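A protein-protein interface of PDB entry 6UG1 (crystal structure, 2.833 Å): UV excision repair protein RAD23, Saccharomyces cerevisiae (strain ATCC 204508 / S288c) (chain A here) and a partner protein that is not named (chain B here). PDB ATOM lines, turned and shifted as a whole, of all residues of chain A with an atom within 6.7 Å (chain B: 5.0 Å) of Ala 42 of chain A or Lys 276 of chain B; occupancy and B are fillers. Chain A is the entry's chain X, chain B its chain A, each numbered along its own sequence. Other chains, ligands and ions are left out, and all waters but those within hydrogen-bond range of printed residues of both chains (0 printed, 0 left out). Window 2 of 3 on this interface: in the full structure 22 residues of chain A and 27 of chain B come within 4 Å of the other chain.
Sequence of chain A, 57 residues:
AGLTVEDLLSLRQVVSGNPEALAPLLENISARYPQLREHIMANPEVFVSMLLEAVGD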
ATOM      1  N   ARG A  37      13.951  11.600 -15.909  1.00  0.00           N
ATOM      2  CA  ARG A  37      13.325  12.002 -17.166  1.00  0.00           C
ATOM      3  C   ARG A  37      12.295  13.111 -16.961  1.00  0.00           C
ATOM      4  O   ARG A  37      12.459  14.223 -17.480  1.00  0.00           O
ATOM      5  CB  ARG A  37      12.587  10.799 -17.749  1.00  0.00           C
ATOM      6  CG  ARG A  37      11.362  11.240 -18.557  1.00  0.00           C
ATOM      7  CD  ARG A  37      10.774  10.280 -19.533  1.00  0.00           C
ATOM      8  NE  ARG A  37      11.470   9.677 -20.656  1.00  0.00           N
ATOM      9  CZ  ARG A  37      11.257   9.979 -21.934  1.00  0.00           C
ATOM     10  NH1 ARG A  37      10.356  10.898 -22.300  1.00  0.00           N
ATOM     11  NH2 ARG A  37      11.864   9.261 -22.845  1.00  0.00           N
ATOM     12  N   GLU A  38      11.247  12.848 -16.139  1.00  0.00           N
ATOM     13  CA  GLU A  38      10.167  13.832 -16.047  1.00  0.00           C
ATOM     14  C   GLU A  38      10.583  15.077 -15.325  1.00  0.00           C
ATOM     15  O   GLU A  38      10.121  16.181 -15.669  1.00  0.00           O
ATOM     16  CB  GLU A  38       9.044  13.264 -15.201  1.00  0.00           C
ATOM     17  CG  GLU A  38       8.005  12.466 -15.863  1.00  0.00           C
ATOM     18  CD  GLU A  38       7.270  11.667 -14.793  1.00  0.00           C
ATOM     19  OE1 GLU A  38       7.392  12.057 -13.600  1.00  0.00           O
ATOM     20  OE2 GLU A  38       6.593  10.664 -15.122  1.00  0.00           O
ATOM     21  N   HIS A  39      11.597  14.909 -14.488  1.00  0.00           N
ATOM     22  CA  HIS A  39      12.237  15.985 -13.760  1.00  0.00           C
ATOM     23  C   HIS A  39      12.813  16.959 -14.748  1.00  0.00           C
ATOM     24  O   HIS A  39      12.635  18.178 -14.654  1.00  0.00           O
ATOM     25  CB  HIS A  39      13.300  15.418 -12.841  1.00  0.00           C
ATOM     26  CG  HIS A  39      13.786  16.411 -11.867  1.00  0.00           C
ATOM     27  ND1 HIS A  39      15.120  16.597 -11.593  1.00  0.00           N
ATOM     28  CD2 HIS A  39      13.103  17.286 -11.090  1.00  0.00           C
ATOM     29  CE1 HIS A  39      15.240  17.542 -10.680  1.00  0.00           C
ATOM     30  NE2 HIS A  39      14.032  17.982 -10.363  1.00  0.00           N
ATOM     31  N   ILE A  40      13.620  16.418 -15.642  1.00  0.00           N
ATOM     32  CA  ILE A  40      14.307  17.209 -16.627  1.00  0.00           C
ATOM     33  C   ILE A  40      13.285  17.985 -17.444  1.00  0.00           C
ATOM     34  O   ILE A  40      13.555  19.110 -17.898  1.00  0.00           O
ATOM     35  CB  ILE A  40      15.099  16.268 -17.539  1.00  0.00           C
ATOM     36  CG1 ILE A  40      16.345  15.751 -16.774  1.00  0.00           C
ATOM     37  CG2 ILE A  40      15.471  17.003 -18.813  1.00  0.00           C
ATOM     38  CD1 ILE A  40      17.426  16.595 -16.546  1.00  0.00           C
ATOM     39  N   MET A  41      12.072  17.442 -17.594  1.00  0.00           N
ATOM     40  CA  MET A  41      11.099  18.160 -18.412  1.00  0.00           C
ATOM     41  C   MET A  41      10.469  19.291 -17.641  1.00  0.00           C
ATOM     42  O   MET A  41      10.212  20.357 -18.191  1.00  0.00           O
ATOM     43  CB  MET A  41       9.996  17.208 -18.846  1.00  0.00           C
ATOM     44  CG  MET A  41      10.568  16.009 -19.528  1.00  0.00           C
ATOM     45  SD  MET A  41      11.301  16.431 -21.070  1.00  0.00           S
ATOM     46  CE  MET A  41      10.999  14.893 -21.913  1.00  0.00           C
ATOM     47  N   ALA A  42      10.215  19.062 -16.365  1.00  0.00           N
ATOM     48  CA  ALA A  42       9.542  20.052 -15.548  1.00  0.00           C
ATOM     49  C   ALA A  42      10.505  21.122 -15.051  1.00  0.00           C
ATOM     50  O   ALA A  42      10.220  22.326 -15.117  1.00  0.00           O
ATOM     51  CB  ALA A  42       8.854  19.337 -14.393  1.00  0.00           C
ATOM     52  N   ASN A  43      11.642  20.681 -14.528  1.00  0.00           N
ATOM     53  CA  ASN A  43      12.535  21.496 -13.712  1.00  0.00           C
ATOM     54  C   ASN A  43      13.987  21.324 -14.116  1.00  0.00           C
ATOM     55  O   ASN A  43      14.756  20.654 -13.434  1.00  0.00           O
ATOM     56  CB  ASN A  43      12.296  21.107 -12.263  1.00  0.00           C
ATOM     57  CG  ASN A  43      10.870  21.261 -11.912  1.00  0.00           C
ATOM     58  OD1 ASN A  43      10.359  22.385 -11.937  1.00  0.00           O
ATOM     59  ND2 ASN A  43      10.178  20.152 -11.712  1.00  0.00           N
ATOM     60  N   PRO A  44      14.325  21.700 -15.330  1.00  0.00           N
ATOM     61  CA  PRO A  44      15.729  21.605 -15.766  1.00  0.00           C
ATOM     62  C   PRO A  44      16.694  22.421 -14.902  1.00  0.00           C
ATOM     63  O   PRO A  44      17.865  22.048 -14.722  1.00  0.00           O
ATOM     64  CB  PRO A  44      15.664  22.140 -17.194  1.00  0.00           C
ATOM     65  CG  PRO A  44      14.172  22.200 -17.527  1.00  0.00           C
ATOM     66  CD  PRO A  44      13.440  22.316 -16.328  1.00  0.00           C
ATOM     67  N   GLU A  45      16.264  23.630 -14.526  1.00  0.00           N
ATOM     68  CA  GLU A  45      17.107  24.554 -13.799  1.00  0.00           C
ATOM     69  C   GLU A  45      17.632  23.981 -12.488  1.00  0.00           C
ATOM     70  O   GLU A  45      18.776  24.273 -12.104  1.00  0.00           O
ATOM     71  CB  GLU A  45      16.307  25.839 -13.518  1.00  0.00           C
ATOM     72  CG  GLU A  45      15.043  25.729 -12.627  1.00  0.00           C
ATOM     73  CD  GLU A  45      13.817  25.107 -13.311  1.00  0.00           C
ATOM     74  OE1 GLU A  45      13.720  25.260 -14.541  1.00  0.00           O
ATOM     75  OE2 GLU A  45      12.937  24.487 -12.645  1.00  0.00           O
ATOM     76  N   VAL A  48      20.438  21.623 -13.621  1.00  0.00           N
ATOM     77  CA  VAL A  48      21.558  22.520 -13.927  1.00  0.00           C
ATOM     78  C   VAL A  48      22.307  22.883 -12.639  1.00  0.00           C
ATOM     79  O   VAL A  48      23.511  22.580 -12.512  1.00  0.00           O
ATOM     80  CB  VAL A  48      21.095  23.789 -14.689  1.00  0.00           C
ATOM     81  CG1 VAL A  48      22.206  24.729 -14.852  1.00  0.00           C
ATOM     82  CG2 VAL A  48      20.603  23.463 -16.125  1.00  0.00           C
ATOM     83  N   GLU B 271      10.062  26.342 -25.855  1.00  0.00           N
ATOM     84  CA  GLU B 271      10.533  27.666 -25.490  1.00  0.00           C
ATOM     85  C   GLU B 271      10.616  27.899 -23.981  1.00  0.00           C
ATOM     86  O   GLU B 271      11.574  28.494 -23.469  1.00  0.00           O
ATOM     87  CB  GLU B 271       9.638  28.706 -26.117  1.00  0.00           C
ATOM     88  CG  GLU B 271      10.153  30.057 -25.755  1.00  0.00           C
ATOM     89  CD  GLU B 271      10.834  30.716 -26.929  1.00  0.00           C
ATOM     90  OE1 GLU B 271      10.603  30.283 -28.104  1.00  0.00           O
ATOM     91  OE2 GLU B 271      11.737  31.549 -26.634  1.00  0.00           O
ATOM     92  N   LYS B 272       9.577  27.538 -23.263  1.00  0.00           N
ATOM     93  CA  LYS B 272       9.604  27.816 -21.835  1.00  0.00           C
ATOM     94  C   LYS B 272      10.705  27.025 -21.164  1.00  0.00           C
ATOM     95  O   LYS B 272      11.441  27.569 -20.331  1.00  0.00           O
ATOM     96  CB  LYS B 272       8.254  27.519 -21.194  1.00  0.00           C
ATOM     97  CG  LYS B 272       7.196  28.455 -21.725  1.00  0.00           C
ATOM     98  CD  LYS B 272       7.312  29.864 -21.123  1.00  0.00           C
ATOM     99  CE  LYS B 272       5.934  30.524 -21.055  1.00  0.00           C
ATOM    100  NZ  LYS B 272       5.404  30.821 -22.412  1.00  0.00           N
ATOM    101  N   TRP B 273      10.897  25.775 -21.603  1.00  0.00           N
ATOM    102  CA  TRP B 273      11.970  24.951 -21.064  1.00  0.00           C
ATOM    103  C   TRP B 273      13.357  25.537 -21.372  1.00  0.00           C
ATOM    104  O   TRP B 273      14.195  25.778 -20.480  1.00  0.00           O
ATOM    105  CB  TRP B 273      11.832  23.583 -21.726  1.00  0.00           C
ATOM    106  CG  TRP B 273      12.846  22.498 -21.340  1.00  0.00           C
ATOM    107  CD1 TRP B 273      12.700  21.612 -20.342  1.00  0.00           C
ATOM    108  CD2 TRP B 273      14.165  22.259 -21.883  1.00  0.00           C
ATOM    109  NE1 TRP B 273      13.810  20.795 -20.239  1.00  0.00           N
ATOM    110  CE2 TRP B 273      14.723  21.181 -21.175  1.00  0.00           C
ATOM    111  CE3 TRP B 273      14.903  22.817 -22.914  1.00  0.00           C
ATOM    112  CZ2 TRP B 273      15.973  20.651 -21.482  1.00  0.00           C
ATOM    113  CZ3 TRP B 273      16.135  22.286 -23.200  1.00  0.00           C
ATOM    114  CH2 TRP B 273      16.658  21.236 -22.508  1.00  0.00           C
ATOM    115  N   PHE B 274      13.589  25.826 -22.637  1.00  0.00           N
ATOM    116  CA  PHE B 274      14.819  26.455 -23.033  1.00  0.00           C
ATOM    117  C   PHE B 274      15.089  27.716 -22.208  1.00  0.00           C
ATOM    118  O   PHE B 274      16.213  27.932 -21.742  1.00  0.00           O
ATOM    119  CB  PHE B 274      14.690  26.827 -24.484  1.00  0.00           C
ATOM    120  CG  PHE B 274      15.959  27.134 -25.130  1.00  0.00           C
ATOM    121  CD1 PHE B 274      16.977  26.161 -25.132  1.00  0.00           C
ATOM    122  CD2 PHE B 274      16.225  28.434 -25.547  1.00  0.00           C
ATOM    123  CE1 PHE B 274      18.162  26.411 -25.683  1.00  0.00           C
ATOM    124  CE2 PHE B 274      17.428  28.721 -26.067  1.00  0.00           C
ATOM    125  CZ  PHE B 274      18.418  27.725 -26.148  1.00  0.00           C
ATOM    126  N   ARG B 275      14.081  28.584 -22.019  1.00  0.00           N
ATOM    127  CA  ARG B 275      14.375  29.814 -21.272  1.00  0.00           C
ATOM    128  C   ARG B 275      14.753  29.464 -19.839  1.00  0.00           C
ATOM    129  O   ARG B 275      15.544  30.187 -19.209  1.00  0.00           O
ATOM    130  CB  ARG B 275      13.238  30.835 -21.323  1.00  0.00           C
ATOM    131  CG  ARG B 275      13.143  31.591 -22.638  1.00  0.00           C
ATOM    132  CD  ARG B 275      14.416  32.450 -23.003  1.00  0.00           C
ATOM    133  NE  ARG B 275      14.287  33.183 -24.274  1.00  0.00           N
ATOM    134  CZ  ARG B 275      13.820  34.437 -24.398  1.00  0.00           C
ATOM    135  NH1 ARG B 275      13.393  35.112 -23.330  1.00  0.00           N
ATOM    136  NH2 ARG B 275      13.740  35.028 -25.595  1.00  0.00           N
ATOM    137  N   LYS B 276      14.206  28.368 -19.307  1.00  0.00           N
ATOM    138  CA  LYS B 276      14.547  28.003 -17.933  1.00  0.00           C
ATOM    139  C   LYS B 276      16.061  27.744 -17.833  1.00  0.00           C
ATOM    140  O   LYS B 276      16.715  28.150 -16.855  1.00  0.00           O
ATOM    141  CB  LYS B 276      13.742  26.744 -17.549  1.00  0.00           C
ATOM    142  CG  LYS B 276      12.285  26.965 -17.300  1.00  0.00           C
ATOM    143  CD  LYS B 276      11.614  25.688 -16.806  1.00  0.00           C
ATOM    144  CE  LYS B 276      10.067  25.781 -16.948  1.00  0.00           C
ATOM    145  NZ  LYS B 276       9.292  24.701 -16.351  1.00  0.00           N
ATOM    146  N   VAL B 277      16.617  27.044 -18.837  1.00  0.00           N
ATOM    147  CA  VAL B 277      18.054  26.713 -18.862  1.00  0.00           C
ATOM    148  C   VAL B 277      18.915  27.953 -19.091  1.00  0.00           C
ATOM    149  O   VAL B 277      19.998  28.098 -18.518  1.00  0.00           O
ATOM    150  CB  VAL B 277      18.405  25.568 -19.834  1.00  0.00           C
ATOM    151  CG1 VAL B 277      17.345  24.419 -19.742  1.00  0.00           C
ATOM    152  CG2 VAL B 277      18.518  26.023 -21.123  1.00  0.00           C
ATOM    153  N   ILE B 278      18.524  28.813 -19.992  1.00  0.00           N
ATOM    154  CA  ILE B 278      19.389  29.977 -20.190  1.00  0.00           C
ATOM    155  C   ILE B 278      19.441  30.785 -18.926  1.00  0.00           C
ATOM    156  O   ILE B 278      20.518  31.141 -18.445  1.00  0.00           O
ATOM    157  CB  ILE B 278      18.868  30.868 -21.349  1.00  0.00           C
ATOM    158  CG1 ILE B 278      18.854  30.093 -22.691  1.00  0.00           C
ATOM    159  CG2 ILE B 278      19.619  32.224 -21.373  1.00  0.00           C
ATOM    160  CD1 ILE B 278      20.146  29.956 -23.362  1.00  0.00           C
ATOM    161  N   THR B 279      18.309  30.954 -18.292  1.00  0.00           N
ATOM    162  CA  THR B 279      18.311  31.746 -17.084  1.00  0.00           C
ATOM    163  C   THR B 279      19.128  31.042 -16.003  1.00  0.00           C
ATOM    164  O   THR B 279      19.842  31.682 -15.225  1.00  0.00           O
ATOM    165  CB  THR B 279      16.873  32.043 -16.718  1.00  0.00           C
ATOM    166  OG1 THR B 279      16.382  32.947 -17.733  1.00  0.00           O
ATOM    167  CG2 THR B 279      16.775  32.640 -15.359  1.00  0.00           C
ATOM    168  N   ALA B 280      19.025  29.715 -15.958  1.00  0.00           N
ATOM    169  CA  ALA B 280      19.852  28.905 -15.080  1.00  0.00           C
ATOM    170  C   ALA B 280      21.343  29.155 -15.284  1.00  0.00           C
ATOM    171  O   ALA B 280      22.152  28.870 -14.391  1.00  0.00           O
ATOM    172  CB  ALA B 280      19.588  27.424 -15.361  1.00  0.00           C
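The side-chain amide oxygen (OD1) of Asn 43 of chain A lies close to the side-chain carboxylate (OE2) of Glu 45 of chain A (3.4 Å).
The backbone carbonyl oxygen (O) of Ala 42 of chain A lies within hydrogen-bond range of the side-chain amino group (NZ) of Lys 276 of chain B, 2.8 Å away.
NE1 of Trp 273 of chain B is in hydrogen-bond range of O of Ile 40 of chain A (2.9 Å).
Of the 10 printed residues of chain B, 4 touch a printed residue of chain A.
Printed residues of chain B that touch a printed residue of chain A: Trp 273, Lys 276, Val 277 and Ala 280.
Hydrophobic or aromatic side chains of chain B within 4 Å of the printed part of chain A: Trp 273, Val 277 and Ala 280.
Printed residues of chain A that touch a printed residue of chain B: Ile 40, Met 41, Ala 42, Pro 44, Glu 45 and Val 48.
Hydrophobic or aromatic side chains of chain A that line the printed part of chain B: Pro 44 and Val 48.
Among the printed residues, no Asp or Glu carboxylate lies within 4 Å of a Lys or Arg side-chain nitrogen of the other chain.
Trp 273 of chain B touches Met 41 of chain A.
NE1 of Trp 273 of chain B touches CG of Pro 44 of chain A, 3.1 Å away.
Lys 276 of chain B touches Pro 44 of chain A.
Pro 44 of chain A touches Val 277 of chain B.
CD of Lys 276 of chain B touches OE1 of Glu 45 of chain A, 3.1 Å away.
Ala 280 of chain B touches Val 48 of chain A (CB to CG1, 3.8 Å).
Printed residues of chain B within 4 Å of Ile 40 of chain A: Trp 273.
Ala 42 of chain A touches just one residue of chain B: Lys 276.
Of the printed residues of chain B, Pro 44 of chain A touches Trp 273 (3.1 Å), Lys 276 (3.9 Å) and Val 277 (3.8 Å).
Printed residues of chain B within 4 Å of Glu 45 of chain A: Lys 276 (3.1 Å).
Of the printed residues of chain B, Val 48 of chain A touches Ala 280 (3.8 Å).
Of chain A, only Ala 42, Pro 44 and Glu 45 come within 4 Å of Lys 276 of chain B.
The nearest printed residue of chain B that does not touch Ala 42 of chain A is Trp 273 of chain B (5.3 Å).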
